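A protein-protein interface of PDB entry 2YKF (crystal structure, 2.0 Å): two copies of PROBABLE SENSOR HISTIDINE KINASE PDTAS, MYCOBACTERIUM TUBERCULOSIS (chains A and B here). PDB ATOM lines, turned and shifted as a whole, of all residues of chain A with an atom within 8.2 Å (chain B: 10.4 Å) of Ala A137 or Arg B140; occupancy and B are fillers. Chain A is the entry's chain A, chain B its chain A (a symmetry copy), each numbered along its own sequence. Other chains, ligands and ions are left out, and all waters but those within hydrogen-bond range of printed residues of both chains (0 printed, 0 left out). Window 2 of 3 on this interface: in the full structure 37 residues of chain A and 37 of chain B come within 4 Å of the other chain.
Gly A64 touches Arg B139, and with the chains exchanged Arg A139 touches Gly B64.
Pro A65 touches Arg B139, and with the chains exchanged Arg A139 touches Pro B65.
Ala A137 touches Arg B140, and with the chains exchanged Arg A140 touches Ala B137.
Positions printed for both chains: 64, 65, 132, 133, 134, 135, 136, 137, 138, 139, 140 and 149.
Of the 6 pairs that touch across the chains among the printed residues, 6 have their exchanged pair printed and touching as well.
Among the printed residues, pairs that only touch across the chains: Ala A137 with Arg B140 (3.1 Å), Arg A140 with Ala B137 (3.1 Å), Arg A139 with Gly B64 (3.3 Å), Gly A64 with Arg B139 (3.3 Å), Arg A139 with Pro B65 (3.5 Å) and Pro A65 with Arg B139 (3.5 Å).
No residue of chain B comes within 4 Å of Pro A133.
No residue of chain B comes within 4 Å of Ala A136.
Of the printed residues of chain A, Ala B137 touches Arg A140 (3.1 Å).
Printed residues of chain B within 4 Å of Arg A139: Gly B64 and Pro B65.
Of the printed residues of chain B, Arg A140 touches Ala B137 (3.1 Å).
Ser B141 touches none of the printed residues of chain A.
Thr B63 touches none of the printed residues of chain A.
The nearest printed residue of chain B that does not touch Arg A139 is Thr B63 (4.3 Å).
Of the 13 printed residues of chain A, 5 touch a printed residue of chain B.
Printed residues of chain A that touch a printed residue of chain B: Gly A64, Pro A65, Ala A137, Arg A139 and Arg A140.
Of the 24 printed residues of chain B, 5 touch a printed residue of chain A.
Printed residues of chain B that touch a printed residue of chain A: Gly B64, Pro B65, Ala B137, Arg B139 and Arg B140.
Hydrophobic or aromatic side chains of chain B within 4 Å of the printed part of chain A: Pro B65 and Ala B137.
O of Arg B139 sits at hydrogen-bond distance from NH2 of Arg B149, 2.7 Å away.
O of Thr B63 sits at hydrogen-bond distance from NH2 of Arg B139 (3.1 Å).
The backbone carbonyl oxygen (O) of Arg A139 lies within hydrogen-bond range of the guanidinium group (NH2) of Arg A149, at 2.7 Å.
The side-chain carboxylate (OE2) of Glu B145 is in salt-bridge range of the guanidinium group (NH1) of Arg B139, 2.8 Å away.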
ATOM      1  N   GLY A  64     -16.202  -6.029 -29.889  1.00  0.00           N
ATOM      2  CA  GLY A  64     -16.030  -7.301 -29.132  1.00  0.00           C
ATOM      3  C   GLY A  64     -14.748  -7.301 -28.330  1.00  0.00           C
ATOM      4  O   GLY A  64     -13.940  -6.354 -28.429  1.00  0.00           O
ATOM      5  N   PRO A  65     -14.512  -8.361 -27.526  1.00  0.00           N
ATOM      6  CA  PRO A  65     -13.227  -8.410 -26.746  1.00  0.00           C
ATOM      7  C   PRO A  65     -11.962  -8.444 -27.569  1.00  0.00           C
ATOM      8  O   PRO A  65     -11.949  -9.014 -28.643  1.00  0.00           O
ATOM      9  CB  PRO A  65     -13.347  -9.739 -25.958  1.00  0.00           C
ATOM     10  CG  PRO A  65     -14.336 -10.541 -26.692  1.00  0.00           C
ATOM     11  CD  PRO A  65     -15.359  -9.550 -27.238  1.00  0.00           C
ATOM     12  N   VAL A  67      -7.998  -9.820 -28.042  1.00  0.00           N
ATOM     13  CA  VAL A  67      -7.165 -10.966 -27.641  1.00  0.00           C
ATOM     14  C   VAL A  67      -5.735 -10.509 -27.609  1.00  0.00           C
ATOM     15  O   VAL A  67      -4.819 -11.287 -27.315  1.00  0.00           O
ATOM     16  CB  VAL A  67      -7.381 -12.194 -28.545  1.00  0.00           C
ATOM     17  CG1 VAL A  67      -8.891 -12.602 -28.448  1.00  0.00           C
ATOM     18  CG2 VAL A  67      -6.921 -11.914 -30.021  1.00  0.00           C
ATOM     19  N   GLN A 132      -8.205 -12.831 -33.328  1.00  0.00           N
ATOM     20  CA  GLN A 132      -9.530 -12.807 -32.785  1.00  0.00           C
ATOM     21  C   GLN A 132      -9.799 -13.983 -31.884  1.00  0.00           C
ATOM     22  O   GLN A 132      -9.019 -14.935 -31.900  1.00  0.00           O
ATOM     23  CB  GLN A 132     -10.528 -12.761 -33.934  1.00  0.00           C
ATOM     24  CG  GLN A 132     -10.659 -14.055 -34.731  1.00  0.00           C
ATOM     25  CD  GLN A 132     -11.473 -13.836 -36.010  1.00  0.00           C
ATOM     26  OE1 GLN A 132     -12.621 -13.362 -35.969  1.00  0.00           O
ATOM     27  NE2 GLN A 132     -10.873 -14.164 -37.146  1.00  0.00           N
ATOM     28  N   PRO A 133     -10.891 -13.923 -31.091  1.00  0.00           N
ATOM     29  CA  PRO A 133     -11.143 -14.975 -30.115  1.00  0.00           C
ATOM     30  C   PRO A 133     -11.248 -16.332 -30.765  1.00  0.00           C
ATOM     31  O   PRO A 133     -11.651 -16.435 -31.949  1.00  0.00           O
ATOM     32  CB  PRO A 133     -12.474 -14.562 -29.494  1.00  0.00           C
ATOM     33  CG  PRO A 133     -12.535 -13.063 -29.698  1.00  0.00           C
ATOM     34  CD  PRO A 133     -11.962 -12.902 -31.057  1.00  0.00           C
ATOM     35  N   GLU A 134     -10.808 -17.362 -30.034  1.00  0.00           N
ATOM     36  CA  GLU A 134     -10.968 -18.759 -30.495  1.00  0.00           C
ATOM     37  C   GLU A 134     -12.462 -19.020 -30.699  1.00  0.00           C
ATOM     38  O   GLU A 134     -13.308 -18.352 -30.045  1.00  0.00           O
ATOM     39  CB  GLU A 134     -10.301 -19.794 -29.555  1.00  0.00           C
ATOM     40  CG  GLU A 134     -10.770 -19.813 -28.094  1.00  0.00           C
ATOM     41  CD  GLU A 134     -10.676 -21.231 -27.445  1.00  0.00           C
ATOM     42  OE1 GLU A 134     -10.215 -22.201 -28.126  1.00  0.00           O
ATOM     43  OE2 GLU A 134     -11.091 -21.373 -26.259  1.00  0.00           O
ATOM     44  N   LEU A 135     -12.787 -19.952 -31.610  1.00  0.00           N
ATOM     45  CA  LEU A 135     -14.171 -20.098 -32.146  1.00  0.00           C
ATOM     46  C   LEU A 135     -15.420 -20.060 -31.189  1.00  0.00           C
ATOM     47  O   LEU A 135     -16.348 -19.292 -31.437  1.00  0.00           O
ATOM     48  CB  LEU A 135     -14.252 -21.212 -33.230  1.00  0.00           C
ATOM     49  CG  LEU A 135     -13.687 -20.865 -34.649  1.00  0.00           C
ATOM     50  CD1 LEU A 135     -12.957 -22.046 -35.355  1.00  0.00           C
ATOM     51  CD2 LEU A 135     -14.745 -20.277 -35.608  1.00  0.00           C
ATOM     52  N   ALA A 136     -15.424 -20.816 -30.091  1.00  0.00           N
ATOM     53  CA  ALA A 136     -16.556 -20.760 -29.137  1.00  0.00           C
ATOM     54  C   ALA A 136     -16.700 -19.453 -28.282  1.00  0.00           C
ATOM     55  O   ALA A 136     -17.738 -19.244 -27.611  1.00  0.00           O
ATOM     56  CB  ALA A 136     -16.573 -22.013 -28.228  1.00  0.00           C
ATOM     57  N   ALA A 137     -15.680 -18.595 -28.284  1.00  0.00           N
ATOM     58  CA  ALA A 137     -15.736 -17.344 -27.505  1.00  0.00           C
ATOM     59  C   ALA A 137     -16.178 -16.133 -28.341  1.00  0.00           C
ATOM     60  O   ALA A 137     -16.294 -15.036 -27.815  1.00  0.00           O
ATOM     61  CB  ALA A 137     -14.374 -17.056 -26.865  1.00  0.00           C
ATOM     62  N   ARG A 138     -16.368 -16.311 -29.649  1.00  0.00           N
ATOM     63  CA  ARG A 138     -16.632 -15.153 -30.502  1.00  0.00           C
ATOM     64  C   ARG A 138     -18.096 -14.796 -30.737  1.00  0.00           C
ATOM     65  O   ARG A 138     -19.010 -15.605 -30.518  1.00  0.00           O
ATOM     66  CB  ARG A 138     -15.807 -15.141 -31.808  1.00  0.00           C
ATOM     67  CG  ARG A 138     -15.981 -16.280 -32.739  1.00  0.00           C
ATOM     68  CD  ARG A 138     -14.604 -16.721 -33.213  1.00  0.00           C
ATOM     69  NE  ARG A 138     -14.346 -16.489 -34.629  1.00  0.00           N
ATOM     70  CZ  ARG A 138     -13.236 -16.882 -35.267  1.00  0.00           C
ATOM     71  NH1 ARG A 138     -12.256 -17.521 -34.625  1.00  0.00           N
ATOM     72  NH2 ARG A 138     -13.094 -16.634 -36.563  1.00  0.00           N
ATOM     73  N   ARG A 139     -18.291 -13.540 -31.135  1.00  0.00           N
ATOM     74  CA  ARG A 139     -19.600 -13.037 -31.523  1.00  0.00           C
ATOM     75  C   ARG A 139     -20.276 -13.999 -32.465  1.00  0.00           C
ATOM     76  O   ARG A 139     -19.885 -14.079 -33.635  1.00  0.00           O
ATOM     77  CB  ARG A 139     -19.438 -11.703 -32.220  1.00  0.00           C
ATOM     78  CG  ARG A 139     -19.667 -10.614 -31.309  1.00  0.00           C
ATOM     79  CD  ARG A 139     -21.077 -10.125 -31.382  1.00  0.00           C
ATOM     80  NE  ARG A 139     -20.934  -8.741 -31.073  1.00  0.00           N
ATOM     81  CZ  ARG A 139     -21.721  -7.754 -31.439  1.00  0.00           C
ATOM     82  NH1 ARG A 139     -22.836  -7.942 -32.168  1.00  0.00           N
ATOM     83  NH2 ARG A 139     -21.327  -6.545 -31.067  1.00  0.00           N
ATOM     84  N   ARG A 140     -21.262 -14.726 -31.928  1.00  0.00           N
ATOM     85  CA  ARG A 140     -22.116 -15.668 -32.665  1.00  0.00           C
ATOM     86  C   ARG A 140     -22.710 -15.020 -33.917  1.00  0.00           C
ATOM     87  O   ARG A 140     -23.148 -13.843 -33.851  1.00  0.00           O
ATOM     88  CB  ARG A 140     -23.205 -16.185 -31.726  1.00  0.00           C
ATOM     89  CG  ARG A 140     -22.591 -16.828 -30.467  1.00  0.00           C
ATOM     90  CD  ARG A 140     -23.222 -18.184 -30.122  1.00  0.00           C
ATOM     91  NE  ARG A 140     -24.288 -18.065 -29.118  1.00  0.00           N
ATOM     92  CZ  ARG A 140     -24.087 -17.867 -27.808  1.00  0.00           C
ATOM     93  NH1 ARG A 140     -22.851 -17.749 -27.312  1.00  0.00           N
ATOM     94  NH2 ARG A 140     -25.129 -17.782 -26.981  1.00  0.00           N
ATOM     95  N   ARG A 149     -18.879  -8.882 -41.126  1.00  0.00           N
ATOM     96  CA  ARG A 149     -17.731  -9.681 -41.508  1.00  0.00           C
ATOM     97  C   ARG A 149     -17.562  -9.709 -43.025  1.00  0.00           C
ATOM     98  O   ARG A 149     -16.455  -9.617 -43.533  1.00  0.00           O
ATOM     99  CB  ARG A 149     -17.875 -11.086 -40.933  1.00  0.00           C
ATOM    100  CG  ARG A 149     -17.961 -11.090 -39.377  1.00  0.00           C
ATOM    101  CD  ARG A 149     -18.126 -12.496 -38.829  1.00  0.00           C
ATOM    102  NE  ARG A 149     -17.733 -12.536 -37.416  1.00  0.00           N
ATOM    103  CZ  ARG A 149     -18.557 -12.822 -36.429  1.00  0.00           C
ATOM    104  NH1 ARG A 149     -19.805 -13.157 -36.689  1.00  0.00           N
ATOM    105  NH2 ARG A 149     -18.129 -12.795 -35.189  1.00  0.00           N
ATOM    106  N   SER B  38     -22.698  -0.918 -20.140  1.00  0.00           N
ATOM    107  CA  SER B  38     -23.570  -1.988 -19.632  1.00  0.00           C
ATOM    108  C   SER B  38     -23.561  -3.221 -20.552  1.00  0.00           C
ATOM    109  O   SER B  38     -24.117  -4.237 -20.174  1.00  0.00           O
ATOM    110  CB  SER B  38     -25.029  -1.526 -19.516  1.00  0.00           C
ATOM    111  OG  SER B  38     -25.177  -0.328 -18.780  1.00  0.00           O
ATOM    112  N   PHE B  39     -23.038  -3.109 -21.798  1.00  0.00           N
ATOM    113  CA  PHE B  39     -23.238  -4.163 -22.805  1.00  0.00           C
ATOM    114  C   PHE B  39     -24.717  -4.539 -22.932  1.00  0.00           C
ATOM    115  O   PHE B  39     -25.064  -5.746 -23.031  1.00  0.00           O
ATOM    116  CB  PHE B  39     -22.405  -5.437 -22.458  1.00  0.00           C
ATOM    117  CG  PHE B  39     -20.965  -5.149 -22.184  1.00  0.00           C
ATOM    118  CD1 PHE B  39     -20.044  -5.126 -23.220  1.00  0.00           C
ATOM    119  CD2 PHE B  39     -20.516  -4.875 -20.906  1.00  0.00           C
ATOM    120  CE1 PHE B  39     -18.714  -4.821 -22.980  1.00  0.00           C
ATOM    121  CE2 PHE B  39     -19.198  -4.544 -20.676  1.00  0.00           C
ATOM    122  CZ  PHE B  39     -18.284  -4.544 -21.706  1.00  0.00           C
ATOM    123  N   THR B  63     -20.887  -2.231 -27.928  1.00  0.00           N
ATOM    124  CA  THR B  63     -19.844  -3.142 -27.435  1.00  0.00           C
ATOM    125  C   THR B  63     -20.366  -4.600 -27.329  1.00  0.00           C
ATOM    126  O   THR B  63     -19.644  -5.474 -26.894  1.00  0.00           O
ATOM    127  CB  THR B  63     -19.467  -2.720 -26.020  1.00  0.00           C
ATOM    128  OG1 THR B  63     -20.694  -2.541 -25.293  1.00  0.00           O
ATOM    129  CG2 THR B  63     -18.694  -1.367 -26.062  1.00  0.00           C
ATOM    130  N   GLY B  64     -21.622  -4.857 -27.677  1.00  0.00           N
ATOM    131  CA  GLY B  64     -22.090  -6.270 -27.737  1.00  0.00           C
ATOM    132  C   GLY B  64     -23.385  -6.394 -28.506  1.00  0.00           C
ATOM    133  O   GLY B  64     -23.977  -5.373 -28.917  1.00  0.00           O
ATOM    134  N   PRO B  65     -23.876  -7.636 -28.713  1.00  0.00           N
ATOM    135  CA  PRO B  65     -25.183  -7.790 -29.440  1.00  0.00           C
ATOM    136  C   PRO B  65     -26.383  -7.165 -28.770  1.00  0.00           C
ATOM    137  O   PRO B  65     -26.455  -7.133 -27.557  1.00  0.00           O
ATOM    138  CB  PRO B  65     -25.379  -9.326 -29.485  1.00  0.00           C
ATOM    139  CG  PRO B  65     -24.538  -9.860 -28.405  1.00  0.00           C
ATOM    140  CD  PRO B  65     -23.306  -8.961 -28.348  1.00  0.00           C
ATOM    141  N   GLN B 132     -30.646  -7.370 -21.820  1.00  0.00           N
ATOM    142  CA  GLN B 132     -29.375  -7.881 -22.237  1.00  0.00           C
ATOM    143  C   GLN B 132     -29.400  -9.372 -22.445  1.00  0.00           C
ATOM    144  O   GLN B 132     -30.356 -10.017 -22.015  1.00  0.00           O
ATOM    145  CB  GLN B 132     -28.329  -7.494 -21.200  1.00  0.00           C
ATOM    146  CG  GLN B 132     -28.424  -8.240 -19.874  1.00  0.00           C
ATOM    147  CD  GLN B 132     -27.515  -7.606 -18.816  1.00  0.00           C
ATOM    148  OE1 GLN B 132     -26.299  -7.456 -19.019  1.00  0.00           O
ATOM    149  NE2 GLN B 132     -28.109  -7.217 -17.696  1.00  0.00           N
ATOM    150  N   PRO B 133     -28.363  -9.925 -23.111  1.00  0.00           N
ATOM    151  CA  PRO B 133     -28.383 -11.343 -23.446  1.00  0.00           C
ATOM    152  C   PRO B 133     -28.523 -12.209 -22.219  1.00  0.00           C
ATOM    153  O   PRO B 133     -28.088 -11.810 -21.112  1.00  0.00           O
ATOM    154  CB  PRO B 133     -27.031 -11.562 -24.118  1.00  0.00           C
ATOM    155  CG  PRO B 133     -26.654 -10.198 -24.656  1.00  0.00           C
ATOM    156  CD  PRO B 133     -27.109  -9.291 -23.575  1.00  0.00           C
ATOM    157  N   GLU B 134     -29.203 -13.349 -22.387  1.00  0.00           N
ATOM    158  CA  GLU B 134     -29.308 -14.352 -21.304  1.00  0.00           C
ATOM    159  C   GLU B 134     -27.890 -14.781 -20.920  1.00  0.00           C
ATOM    160  O   GLU B 134     -26.961 -14.699 -21.769  1.00  0.00           O
ATOM    161  CB  GLU B 134     -30.221 -15.550 -21.664  1.00  0.00           C
ATOM    162  CG  GLU B 134     -29.843 -16.365 -22.909  1.00  0.00           C
ATOM    163  CD  GLU B 134     -30.260 -17.865 -22.801  1.00  0.00           C
ATOM    164  OE1 GLU B 134     -30.872 -18.271 -21.762  1.00  0.00           O
ATOM    165  OE2 GLU B 134     -29.946 -18.642 -23.748  1.00  0.00           O
ATOM    166  N   LEU B 135     -27.714 -15.204 -19.658  1.00  0.00           N
ATOM    167  CA  LEU B 135     -26.363 -15.354 -19.046  1.00  0.00           C
ATOM    168  C   LEU B 135     -25.185 -16.037 -19.835  1.00  0.00           C
ATOM    169  O   LEU B 135     -24.108 -15.453 -19.938  1.00  0.00           O
ATOM    170  CB  LEU B 135     -26.454 -15.799 -17.557  1.00  0.00           C
ATOM    171  CG  LEU B 135     -26.860 -14.706 -16.511  1.00  0.00           C
ATOM    172  CD1 LEU B 135     -27.777 -15.225 -15.364  1.00  0.00           C
ATOM    173  CD2 LEU B 135     -25.655 -13.960 -15.899  1.00  0.00           C
ATOM    174  N   ALA B 136     -25.394 -17.210 -20.432  1.00  0.00           N
ATOM    175  CA  ALA B 136     -24.326 -17.853 -21.235  1.00  0.00           C
ATOM    176  C   ALA B 136     -23.964 -17.179 -22.603  1.00  0.00           C
ATOM    177  O   ALA B 136     -22.942 -17.535 -23.236  1.00  0.00           O
ATOM    178  CB  ALA B 136     -24.614 -19.362 -21.426  1.00  0.00           C
ATOM    179  N   ALA B 137     -24.786 -16.237 -23.068  1.00  0.00           N
ATOM    180  CA  ALA B 137     -24.516 -15.556 -24.349  1.00  0.00           C
ATOM    181  C   ALA B 137     -23.793 -14.212 -24.175  1.00  0.00           C
ATOM    182  O   ALA B 137     -23.483 -13.554 -25.157  1.00  0.00           O
ATOM    183  CB  ALA B 137     -25.823 -15.341 -25.119  1.00  0.00           C
ATOM    184  N   ARG B 138     -23.574 -13.774 -22.935  1.00  0.00           N
ATOM    185  CA  ARG B 138     -23.033 -12.430 -22.731  1.00  0.00           C
ATOM    186  C   ARG B 138     -21.518 -12.313 -22.619  1.00  0.00           C
ATOM    187  O   ARG B 138     -20.801 -13.294 -22.373  1.00  0.00           O
ATOM    188  CB  ARG B 138     -23.769 -11.624 -21.637  1.00  0.00           C
ATOM    189  CG  ARG B 138     -23.782 -12.183 -20.265  1.00  0.00           C
ATOM    190  CD  ARG B 138     -25.192 -12.050 -19.711  1.00  0.00           C
ATOM    191  NE  ARG B 138     -25.323 -11.119 -18.597  1.00  0.00           N
ATOM    192  CZ  ARG B 138     -26.453 -10.920 -17.909  1.00  0.00           C
ATOM    193  NH1 ARG B 138     -27.577 -11.573 -18.216  1.00  0.00           N
ATOM    194  NH2 ARG B 138     -26.474 -10.057 -16.901  1.00  0.00           N
ATOM    195  N   ARG B 139     -21.049 -11.090 -22.864  1.00  0.00           N
ATOM    196  CA  ARG B 139     -19.646 -10.742 -22.697  1.00  0.00           C
ATOM    197  C   ARG B 139     -19.132 -11.247 -21.375  1.00  0.00           C
ATOM    198  O   ARG B 139     -19.468 -10.674 -20.332  1.00  0.00           O
ATOM    199  CB  ARG B 139     -19.495  -9.237 -22.737  1.00  0.00           C
ATOM    200  CG  ARG B 139     -19.097  -8.792 -24.045  1.00  0.00           C
ATOM    201  CD  ARG B 139     -17.615  -8.628 -24.142  1.00  0.00           C
ATOM    202  NE  ARG B 139     -17.488  -7.567 -25.085  1.00  0.00           N
ATOM    203  CZ  ARG B 139     -16.497  -6.710 -25.197  1.00  0.00           C
ATOM    204  NH1 ARG B 139     -15.408  -6.748 -24.410  1.00  0.00           N
ATOM    205  NH2 ARG B 139     -16.656  -5.778 -26.125  1.00  0.00           N
ATOM    206  N   ARG B 140     -18.346 -12.327 -21.442  1.00  0.00           N
ATOM    207  CA  ARG B 140     -17.664 -12.951 -20.299  1.00  0.00           C
ATOM    208  C   ARG B 140     -16.884 -11.918 -19.483  1.00  0.00           C
ATOM    209  O   ARG B 140     -16.220 -11.035 -20.084  1.00  0.00           O
ATOM    210  CB  ARG B 140     -16.755 -14.066 -20.815  1.00  0.00           C
ATOM    211  CG  ARG B 140     -17.553 -15.094 -21.640  1.00  0.00           C
ATOM    212  CD  ARG B 140     -17.232 -16.544 -21.257  1.00  0.00           C
ATOM    213  NE  ARG B 140     -16.219 -17.144 -22.136  1.00  0.00           N
ATOM    214  CZ  ARG B 140     -16.445 -17.564 -23.389  1.00  0.00           C
ATOM    215  NH1 ARG B 140     -17.655 -17.449 -23.945  1.00  0.00           N
ATOM    216  NH2 ARG B 140     -15.452 -18.101 -24.099  1.00  0.00           N
ATOM    217  N   SER B 141     -16.965 -12.013 -18.142  1.00  0.00           N
ATOM    218  CA  SER B 141     -16.525 -10.934 -17.252  1.00  0.00           C
ATOM    219  C   SER B 141     -15.023 -10.910 -16.958  1.00  0.00           C
ATOM    220  O   SER B 141     -14.613 -11.188 -15.796  1.00  0.00           O
ATOM    221  CB  SER B 141     -17.285 -10.962 -15.908  1.00  0.00           C
ATOM    222  OG  SER B 141     -18.612 -11.437 -16.031  1.00  0.00           O
ATOM    223  N   GLY B 142     -14.234 -10.547 -17.959  1.00  0.00           N
ATOM    224  CA  GLY B 142     -12.853 -10.196 -17.745  1.00  0.00           C
ATOM    225  C   GLY B 142     -12.788  -8.878 -17.002  1.00  0.00           C
ATOM    226  O   GLY B 142     -13.843  -8.303 -16.637  1.00  0.00           O
ATOM    227  N   HIS B 143     -11.590  -8.397 -16.741  1.00  0.00           N
ATOM    228  CA  HIS B 143     -11.457  -7.124 -16.045  1.00  0.00           C
ATOM    229  C   HIS B 143     -12.114  -5.914 -16.741  1.00  0.00           C
ATOM    230  O   HIS B 143     -12.766  -5.078 -16.061  1.00  0.00           O
ATOM    231  CB  HIS B 143     -10.015  -6.834 -15.719  1.00  0.00           C
ATOM    232  CG  HIS B 143      -9.464  -7.815 -14.734  1.00  0.00           C
ATOM    233  ND1 HIS B 143      -8.291  -8.509 -14.942  1.00  0.00           N
ATOM    234  CD2 HIS B 143     -10.009  -8.319 -13.599  1.00  0.00           C
ATOM    235  CE1 HIS B 143      -8.102  -9.350 -13.939  1.00  0.00           C
ATOM    236  NE2 HIS B 143      -9.121  -9.235 -13.099  1.00  0.00           N
ATOM    237  N   LEU B 144     -11.966  -5.833 -18.065  1.00  0.00           N
ATOM    238  CA  LEU B 144     -12.555  -4.709 -18.841  1.00  0.00           C
ATOM    239  C   LEU B 144     -14.039  -4.708 -18.622  1.00  0.00           C
ATOM    240  O   LEU B 144     -14.622  -3.689 -18.195  1.00  0.00           O
ATOM    241  CB  LEU B 144     -12.247  -4.838 -20.348  1.00  0.00           C
ATOM    242  CG  LEU B 144     -12.831  -3.674 -21.194  1.00  0.00           C
ATOM    243  CD1 LEU B 144     -11.905  -3.460 -22.407  1.00  0.00           C
ATOM    244  CD2 LEU B 144     -14.235  -3.838 -21.694  1.00  0.00           C
ATOM    245  N   GLU B 145     -14.674  -5.860 -18.854  1.00  0.00           N
ATOM    246  CA  GLU B 145     -16.118  -5.928 -18.705  1.00  0.00           C
ATOM    247  C   GLU B 145     -16.591  -5.660 -17.259  1.00  0.00           C
ATOM    248  O   GLU B 145     -17.593  -4.956 -17.027  1.00  0.00           O
ATOM    249  CB  GLU B 145     -16.645  -7.302 -19.218  1.00  0.00           C
ATOM    250  CG  GLU B 145     -16.252  -7.574 -20.740  1.00  0.00           C
ATOM    251  CD  GLU B 145     -14.750  -8.038 -21.023  1.00  0.00           C
ATOM    252  OE1 GLU B 145     -13.888  -8.205 -20.096  1.00  0.00           O
ATOM    253  OE2 GLU B 145     -14.454  -8.242 -22.226  1.00  0.00           O
ATOM    254  N   THR B 146     -15.868  -6.180 -16.277  1.00  0.00           N
ATOM    255  CA  THR B 146     -16.174  -5.769 -14.890  1.00  0.00           C
ATOM    256  C   THR B 146     -16.063  -4.271 -14.643  1.00  0.00           C
ATOM    257  O   THR B 146     -17.020  -3.641 -14.068  1.00  0.00           O
ATOM    258  CB  THR B 146     -15.295  -6.541 -13.879  1.00  0.00           C
ATOM    259  OG1 THR B 146     -15.483  -7.927 -14.126  1.00  0.00           O
ATOM    260  CG2 THR B 146     -15.699  -6.239 -12.537  1.00  0.00           C
ATOM    261  N   ALA B 147     -14.929  -3.662 -15.054  1.00  0.00           N
ATOM    262  CA  ALA B 147     -14.734  -2.183 -14.804  1.00  0.00           C
ATOM    263  C   ALA B 147     -15.839  -1.350 -15.497  1.00  0.00           C
ATOM    264  O   ALA B 147     -16.413  -0.376 -14.931  1.00  0.00           O
ATOM    265  CB  ALA B 147     -13.336  -1.754 -15.342  1.00  0.00           C
ATOM    266  N   TYR B 148     -16.218  -1.798 -16.699  1.00  0.00           N
ATOM    267  CA  TYR B 148     -17.302  -1.084 -17.454  1.00  0.00           C
ATOM    268  C   TYR B 148     -18.642  -1.216 -16.731  1.00  0.00           C
ATOM    269  O   TYR B 148     -19.387  -0.225 -16.598  1.00  0.00           O
ATOM    270  CB  TYR B 148     -17.465  -1.712 -18.837  1.00  0.00           C
ATOM    271  CG  TYR B 148     -16.582  -1.243 -19.936  1.00  0.00           C
ATOM    272  CD1 TYR B 148     -15.358  -0.710 -19.701  1.00  0.00           C
ATOM    273  CD2 TYR B 148     -17.020  -1.345 -21.266  1.00  0.00           C
ATOM    274  CE1 TYR B 148     -14.565  -0.262 -20.775  1.00  0.00           C
ATOM    275  CE2 TYR B 148     -16.239  -0.914 -22.300  1.00  0.00           C
ATOM    276  CZ  TYR B 148     -15.028  -0.405 -22.055  1.00  0.00           C
ATOM    277  OH  TYR B 148     -14.218   0.017 -23.097  1.00  0.00           O
ATOM    278  N   ARG B 149     -18.993  -2.435 -16.328  1.00  0.00           N
ATOM    279  CA  ARG B 149     -20.257  -2.698 -15.669  1.00  0.00           C
ATOM    280  C   ARG B 149     -20.348  -1.958 -14.337  1.00  0.00           C
ATOM    281  O   ARG B 149     -21.385  -1.409 -13.996  1.00  0.00           O
ATOM    282  CB  ARG B 149     -20.434  -4.202 -15.489  1.00  0.00           C
ATOM    283  CG  ARG B 149     -20.434  -4.972 -16.845  1.00  0.00           C
ATOM    284  CD  ARG B 149     -20.589  -6.467 -16.640  1.00  0.00           C
ATOM    285  NE  ARG B 149     -21.056  -7.100 -17.878  1.00  0.00           N
ATOM    286  CZ  ARG B 149     -20.361  -7.987 -18.561  1.00  0.00           C
ATOM    287  NH1 ARG B 149     -19.196  -8.403 -18.107  1.00  0.00           N
ATOM    288  NH2 ARG B 149     -20.840  -8.472 -19.682  1.00  0.00           N
ATOM    289  N   TYR B 194      -8.294   1.497 -12.538  1.00  0.00           N
ATOM    290  CA  TYR B 194      -8.354   0.593 -13.725  1.00  0.00           C
ATOM    291  C   TYR B 194      -8.127   1.431 -14.952  1.00  0.00           C
ATOM    292  O   TYR B 194      -8.682   2.555 -15.029  1.00  0.00           O
ATOM    293  CB  TYR B 194      -9.738  -0.126 -13.862  1.00  0.00           C
ATOM    294  CG  TYR B 194      -9.808  -0.935 -15.143  1.00  0.00           C
ATOM    295  CD1 TYR B 194      -9.150  -2.171 -15.231  1.00  0.00           C
ATOM    296  CD2 TYR B 194     -10.400  -0.400 -16.304  1.00  0.00           C
ATOM    297  CE1 TYR B 194      -9.153  -2.913 -16.401  1.00  0.00           C
ATOM    298  CE2 TYR B 194     -10.413  -1.114 -17.477  1.00  0.00           C
ATOM    299  CZ  TYR B 194      -9.793  -2.361 -17.527  1.00  0.00           C
ATOM    300  OH  TYR B 194      -9.776  -3.049 -18.682  1.00  0.00           O
